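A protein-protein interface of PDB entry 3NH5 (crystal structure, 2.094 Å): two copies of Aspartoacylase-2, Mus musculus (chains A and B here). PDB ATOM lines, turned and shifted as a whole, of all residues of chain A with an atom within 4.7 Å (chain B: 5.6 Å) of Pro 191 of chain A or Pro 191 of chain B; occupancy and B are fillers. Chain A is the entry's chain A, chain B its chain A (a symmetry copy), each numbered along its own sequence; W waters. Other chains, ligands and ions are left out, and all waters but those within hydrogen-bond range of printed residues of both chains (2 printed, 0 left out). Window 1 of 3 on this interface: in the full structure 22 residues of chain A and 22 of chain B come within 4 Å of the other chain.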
ATOM      1  N   THR A 128      -9.776  31.450  -9.049  1.00  0.00           N
ATOM      2  CA  THR A 128      -9.991  30.736  -7.785  1.00  0.00           C
ATOM      3  C   THR A 128     -11.316  31.116  -7.123  1.00  0.00           C
ATOM      4  O   THR A 128     -11.722  30.497  -6.141  1.00  0.00           O
ATOM      5  CB  THR A 128      -8.827  30.949  -6.755  1.00  0.00           C
ATOM      6  OG1 THR A 128      -8.706  32.341  -6.438  1.00  0.00           O
ATOM      7  CG2 THR A 128      -7.497  30.437  -7.328  1.00  0.00           C
ATOM      8  N   PRO A 189     -14.652  27.681  -9.647  1.00  0.00           N
ATOM      9  CA  PRO A 189     -13.324  27.838  -9.035  1.00  0.00           C
ATOM     10  C   PRO A 189     -12.311  26.763  -9.422  1.00  0.00           C
ATOM     11  O   PRO A 189     -12.631  25.587  -9.579  1.00  0.00           O
ATOM     12  CB  PRO A 189     -13.630  27.768  -7.520  1.00  0.00           C
ATOM     13  CG  PRO A 189     -14.786  26.801  -7.426  1.00  0.00           C
ATOM     14  CD  PRO A 189     -15.582  26.945  -8.764  1.00  0.00           C
ATOM     15  N   GLN A 190     -11.064  27.179  -9.569  1.00  0.00           N
ATOM     16  CA  GLN A 190      -9.979  26.233  -9.794  1.00  0.00           C
ATOM     17  C   GLN A 190      -8.691  26.807  -9.222  1.00  0.00           C
ATOM     18  O   GLN A 190      -8.328  27.942  -9.516  1.00  0.00           O
ATOM     19  CB  GLN A 190      -9.801  25.913 -11.295  1.00  0.00           C
ATOM     20  CG  GLN A 190      -8.811  24.794 -11.556  1.00  0.00           C
ATOM     21  CD  GLN A 190      -8.743  24.377 -13.019  1.00  0.00           C
ATOM     22  OE1 GLN A 190      -9.235  23.309 -13.388  1.00  0.00           O
ATOM     23  NE2 GLN A 190      -8.121  25.212 -13.855  1.00  0.00           N
ATOM     24  N   PRO A 191      -7.986  26.020  -8.398  1.00  0.00           N
ATOM     25  CA  PRO A 191      -6.730  26.539  -7.847  1.00  0.00           C
ATOM     26  C   PRO A 191      -5.740  26.788  -8.987  1.00  0.00           C
ATOM     27  O   PRO A 191      -5.712  26.031  -9.943  1.00  0.00           O
ATOM     28  CB  PRO A 191      -6.223  25.390  -6.954  1.00  0.00           C
ATOM     29  CG  PRO A 191      -7.447  24.498  -6.708  1.00  0.00           C
ATOM     30  CD  PRO A 191      -8.252  24.627  -8.003  1.00  0.00           C
ATOM     31  N   GLN A 192      -4.943  27.841  -8.904  1.00  0.00           N
ATOM     32  CA  GLN A 192      -3.822  27.955  -9.818  1.00  0.00           C
ATOM     33  C   GLN A 192      -2.975  26.669  -9.816  1.00  0.00           C
ATOM     34  O   GLN A 192      -2.831  26.001  -8.789  1.00  0.00           O
ATOM     35  CB  GLN A 192      -2.964  29.162  -9.436  1.00  0.00           C
ATOM     36  CG  GLN A 192      -3.669  30.503  -9.630  1.00  0.00           C
ATOM     37  CD  GLN A 192      -2.987  31.634  -8.874  1.00  0.00           C
ATOM     38  OE1 GLN A 192      -2.520  31.455  -7.742  1.00  0.00           O
ATOM     39  NE2 GLN A 192      -2.935  32.807  -9.493  1.00  0.00           N
ATOM     40  N   GLY A 193      -2.419  26.317 -10.972  1.00  0.00           N
ATOM     41  CA  GLY A 193      -1.548  25.161 -11.071  1.00  0.00           C
ATOM     42  C   GLY A 193      -2.249  23.814 -10.942  1.00  0.00           C
ATOM     43  O   GLY A 193      -1.597  22.782 -10.937  1.00  0.00           O
ATOM     44  N   VAL A 194      -3.570  23.808 -10.812  1.00  0.00           N
ATOM     45  CA  VAL A 194      -4.310  22.541 -10.779  1.00  0.00           C
ATOM     46  C   VAL A 194      -5.189  22.466 -12.014  1.00  0.00           C
ATOM     47  O   VAL A 194      -5.846  23.444 -12.367  1.00  0.00           O
ATOM     48  CB  VAL A 194      -5.228  22.408  -9.531  1.00  0.00           C
ATOM     49  CG1 VAL A 194      -6.149  21.216  -9.686  1.00  0.00           C
ATOM     50  CG2 VAL A 194      -4.405  22.303  -8.226  1.00  0.00           C
ATOM     51  N   ASN B  32       3.253  30.137  -0.160  1.00  0.00           N
ATOM     52  CA  ASN B  32       1.939  30.452  -0.733  1.00  0.00           C
ATOM     53  C   ASN B  32       0.809  29.667  -0.079  1.00  0.00           C
ATOM     54  O   ASN B  32      -0.285  29.583  -0.630  1.00  0.00           O
ATOM     55  CB  ASN B  32       1.935  30.218  -2.250  1.00  0.00           C
ATOM     56  CG  ASN B  32       2.360  28.801  -2.625  1.00  0.00           C
ATOM     57  OD1 ASN B  32       2.629  27.971  -1.753  1.00  0.00           O
ATOM     58  ND2 ASN B  32       2.413  28.515  -3.932  1.00  0.00           N
ATOM     59  N   MET B  34      -1.544  29.822   2.764  1.00  0.00           N
ATOM     60  CA  MET B  34      -1.867  31.071   3.428  1.00  0.00           C
ATOM     61  C   MET B  34      -2.298  31.000   4.886  1.00  0.00           C
ATOM     62  O   MET B  34      -2.192  31.997   5.589  1.00  0.00           O
ATOM     63  CB  MET B  34      -2.920  31.853   2.616  1.00  0.00           C
ATOM     64  CG  MET B  34      -2.513  32.062   1.156  1.00  0.00           C
ATOM     65  SD  MET B  34      -1.008  33.048   1.062  1.00  0.00           S
ATOM     66  CE  MET B  34      -1.736  34.684   1.036  1.00  0.00           C
ATOM     67  N   THR B 127      -3.309  22.396   1.479  1.00  0.00           N
ATOM     68  CA  THR B 127      -3.239  21.619   0.246  1.00  0.00           C
ATOM     69  C   THR B 127      -4.420  22.013  -0.646  1.00  0.00           C
ATOM     70  O   THR B 127      -5.472  22.435  -0.139  1.00  0.00           O
ATOM     71  CB  THR B 127      -3.224  20.088   0.527  1.00  0.00           C
ATOM     72  OG1 THR B 127      -3.263  19.352  -0.711  1.00  0.00           O
ATOM     73  CG2 THR B 127      -4.423  19.686   1.356  1.00  0.00           C
ATOM     74  N   THR B 128      -4.235  21.934  -1.965  1.00  0.00           N
ATOM     75  CA  THR B 128      -5.349  22.117  -2.901  1.00  0.00           C
ATOM     76  C   THR B 128      -6.217  20.863  -3.021  1.00  0.00           C
ATOM     77  O   THR B 128      -7.279  20.897  -3.641  1.00  0.00           O
ATOM     78  CB  THR B 128      -4.883  22.554  -4.333  1.00  0.00           C
ATOM     79  OG1 THR B 128      -4.025  21.553  -4.892  1.00  0.00           O
ATOM     80  CG2 THR B 128      -4.135  23.894  -4.273  1.00  0.00           C
ATOM     81  N   PRO B 189      -9.574  21.631   1.154  1.00  0.00           N
ATOM     82  CA  PRO B 189      -8.870  22.283   0.040  1.00  0.00           C
ATOM     83  C   PRO B 189      -8.768  23.803   0.152  1.00  0.00           C
ATOM     84  O   PRO B 189      -9.677  24.489   0.613  1.00  0.00           O
ATOM     85  CB  PRO B 189      -9.725  21.891  -1.188  1.00  0.00           C
ATOM     86  CG  PRO B 189     -11.135  21.836  -0.648  1.00  0.00           C
ATOM     87  CD  PRO B 189     -11.008  21.425   0.854  1.00  0.00           C
ATOM     88  N   GLN B 190      -7.639  24.334  -0.287  1.00  0.00           N
ATOM     89  CA  GLN B 190      -7.472  25.779  -0.371  1.00  0.00           C
ATOM     90  C   GLN B 190      -6.504  26.104  -1.500  1.00  0.00           C
ATOM     91  O   GLN B 190      -5.412  25.550  -1.565  1.00  0.00           O
ATOM     92  CB  GLN B 190      -6.960  26.374   0.960  1.00  0.00           C
ATOM     93  CG  GLN B 190      -6.953  27.891   0.975  1.00  0.00           C
ATOM     94  CD  GLN B 190      -6.590  28.480   2.331  1.00  0.00           C
ATOM     95  OE1 GLN B 190      -7.453  29.008   3.035  1.00  0.00           O
ATOM     96  NE2 GLN B 190      -5.307  28.403   2.697  1.00  0.00           N
ATOM     97  N   PRO B 191      -6.902  27.014  -2.399  1.00  0.00           N
ATOM     98  CA  PRO B 191      -5.982  27.362  -3.487  1.00  0.00           C
ATOM     99  C   PRO B 191      -4.725  28.009  -2.902  1.00  0.00           C
ATOM    100  O   PRO B 191      -4.815  28.742  -1.931  1.00  0.00           O
ATOM    101  CB  PRO B 191      -6.770  28.399  -4.312  1.00  0.00           C
ATOM    102  CG  PRO B 191      -8.236  28.219  -3.894  1.00  0.00           C
ATOM    103  CD  PRO B 191      -8.142  27.806  -2.422  1.00  0.00           C
ATOM    104  N   GLN B 192      -3.561  27.738  -3.470  1.00  0.00           N
ATOM    105  CA  GLN B 192      -2.399  28.533  -3.119  1.00  0.00           C
ATOM    106  C   GLN B 192      -2.698  30.037  -3.255  1.00  0.00           C
ATOM    107  O   GLN B 192      -3.458  30.460  -4.130  1.00  0.00           O
ATOM    108  CB  GLN B 192      -1.216  28.139  -4.005  1.00  0.00           C
ATOM    109  CG  GLN B 192      -0.712  26.718  -3.760  1.00  0.00           C
ATOM    110  CD  GLN B 192       0.158  26.206  -4.900  1.00  0.00           C
ATOM    111  OE1 GLN B 192      -0.119  26.461  -6.078  1.00  0.00           O
ATOM    112  NE2 GLN B 192       1.208  25.472  -4.552  1.00  0.00           N
ATOM    113  N   GLY B 193      -2.105  30.847  -2.384  1.00  0.00           N
ATOM    114  CA  GLY B 193      -2.264  32.288  -2.460  1.00  0.00           C
ATOM    115  C   GLY B 193      -3.644  32.805  -2.076  1.00  0.00           C
ATOM    116  O   GLY B 193      -3.903  33.994  -2.177  1.00  0.00           O
ATOM    117  N   VAL B 194      -4.546  31.925  -1.657  1.00  0.00           N
ATOM    118  CA  VAL B 194      -5.860  32.373  -1.183  1.00  0.00           C
ATOM    119  C   VAL B 194      -5.972  32.054   0.297  1.00  0.00           C
ATOM    120  O   VAL B 194      -5.610  30.957   0.723  1.00  0.00           O
ATOM    121  CB  VAL B 194      -7.039  31.670  -1.914  1.00  0.00           C
ATOM    122  CG1 VAL B 194      -8.345  31.975  -1.208  1.00  0.00           C
ATOM    123  CG2 VAL B 194      -7.110  32.075  -3.403  1.00  0.00           C
ATOM    124  N   LEU B 195      -6.461  33.016   1.067  1.00  0.00           N
ATOM    125  CA  LEU B 195      -6.787  32.809   2.468  1.00  0.00           C
ATOM    126  C   LEU B 195      -8.296  32.756   2.647  1.00  0.00           C
ATOM    127  O   LEU B 195      -8.990  33.765   2.485  1.00  0.00           O
ATOM    128  CB  LEU B 195      -6.221  33.954   3.337  1.00  0.00           C
ATOM    129  CG  LEU B 195      -6.441  33.805   4.847  1.00  0.00           C
ATOM    130  CD1 LEU B 195      -5.766  32.524   5.344  1.00  0.00           C
ATOM    131  CD2 LEU B 195      -5.912  34.999   5.627  1.00  0.00           C
ATOM    132  N   ARG B 196      -8.806  31.586   2.992  1.00  0.00           N
ATOM    133  CA  ARG B 196     -10.213  31.454   3.337  1.00  0.00           C
ATOM    134  C   ARG B 196     -10.430  31.675   4.843  1.00  0.00           C
ATOM    135  O   ARG B 196      -9.709  31.113   5.660  1.00  0.00           O
ATOM    136  CB  ARG B 196     -10.712  30.061   2.949  1.00  0.00           C
ATOM    137  CG  ARG B 196     -10.691  29.769   1.433  1.00  0.00           C
ATOM    138  CD  ARG B 196     -11.200  28.359   1.142  1.00  0.00           C
ATOM    139  NE  ARG B 196     -12.567  28.206   1.633  1.00  0.00           N
ATOM    140  CZ  ARG B 196     -13.659  28.314   0.878  1.00  0.00           C
ATOM    141  NH1 ARG B 196     -13.559  28.549  -0.432  1.00  0.00           N
ATOM    142  NH2 ARG B 196     -14.856  28.173   1.436  1.00  0.00           N
HETATM  143  O   HOH W   1      -4.315  29.476  -6.523  1.00  0.00           O
HETATM  144  O   HOH W   2      -3.054  26.555  -6.131  1.00  0.00           O
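The side-chain amide nitrogen (NE2) of Gln 190 of chain A lies close to the backbone carbonyl oxygen (O) of Val 194 of chain A (3.2 Å).
ND2 of Asn 32 of chain B lies close to NE2 of Gln 192 of chain B (3.3 Å).
NE2 of Gln 190 of chain B sits close to O of Val 194 of chain B (3.2 Å).
Among the printed residues, merely in contact across the chains: Thr 128 of chain A with Pro 191 of chain B (3.7 Å), Thr 128 of chain A with Val 194 of chain B (3.4 Å), Pro 191 of chain A with Thr 128 of chain B (3.7 Å), Pro 191 of chain A with Pro 191 of chain B (3.99 Å), Gln 192 of chain A with Gln 192 of chain B (3.9 Å) and Val 194 of chain A with Thr 128 of chain B (3.4 Å).
Printed residues of chain B within 4 Å of Pro 191 of chain A: Thr 128 (3.7 Å) and Pro 191 (3.99 Å).
Printed residues of chain A within 4 Å of Pro 191 of chain B: Thr 128 and Pro 191.
Printed residues of chain A within 4 Å of Thr 128 of chain B: Pro 191 (3.7 Å) and Val 194 (3.4 Å).
Of the printed residues of chain A, Gln 192 of chain B touches Gln 192.
Of the printed residues of chain B, Gln 192 of chain A touches Gln 192.
The nearest printed residue of chain B that does not touch Pro 191 of chain A is Gln 192 of chain B (5.0 Å).
The nearest printed residue of chain A that does not touch Pro 191 of chain B is Gln 192 of chain A (5.0 Å).
Hydrophobic or aromatic side chains of chain B that line the printed part of chain A: Pro 191 and Val 194.
Of the 7 printed residues of chain A, 4 touch a printed residue of chain B.
Printed residues of chain A that touch a printed residue of chain B: Thr 128, Pro 191, Gln 192 and Val 194.
Hydrophobic or aromatic side chains of chain A within 4 Å of the printed part of chain B: Pro 191 and Val 194.
Among the printed residues, 6 pairs touch across the chains.
Among the printed residues, no Asp or Glu carboxylate lies within 4 Å of a Lys or Arg side-chain nitrogen of the other chain.
Thr 128 of chain A touches Pro 191 of chain B, and with the chains exchanged Pro 191 of chain A touches Thr 128 of chain B.
Thr 128 of chain A touches Val 194 of chain B, and with the chains exchanged Val 194 of chain A touches Thr 128 of chain B.
Pro 191 of chain A touches its own counterpart, Pro 191 of chain B.
Gln 192 of chain B touches its own counterpart, Gln 192 of chain A.
Water W2 lies within hydrogen-bond range of O of Gln 192 of chain A and OE1 of Gln 192 of chain B.
Water W1 lies within hydrogen-bond range of O of Gln 192 of chain B (2.7 Å) and OE1 of Gln 192 of chain A (2.9 Å).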
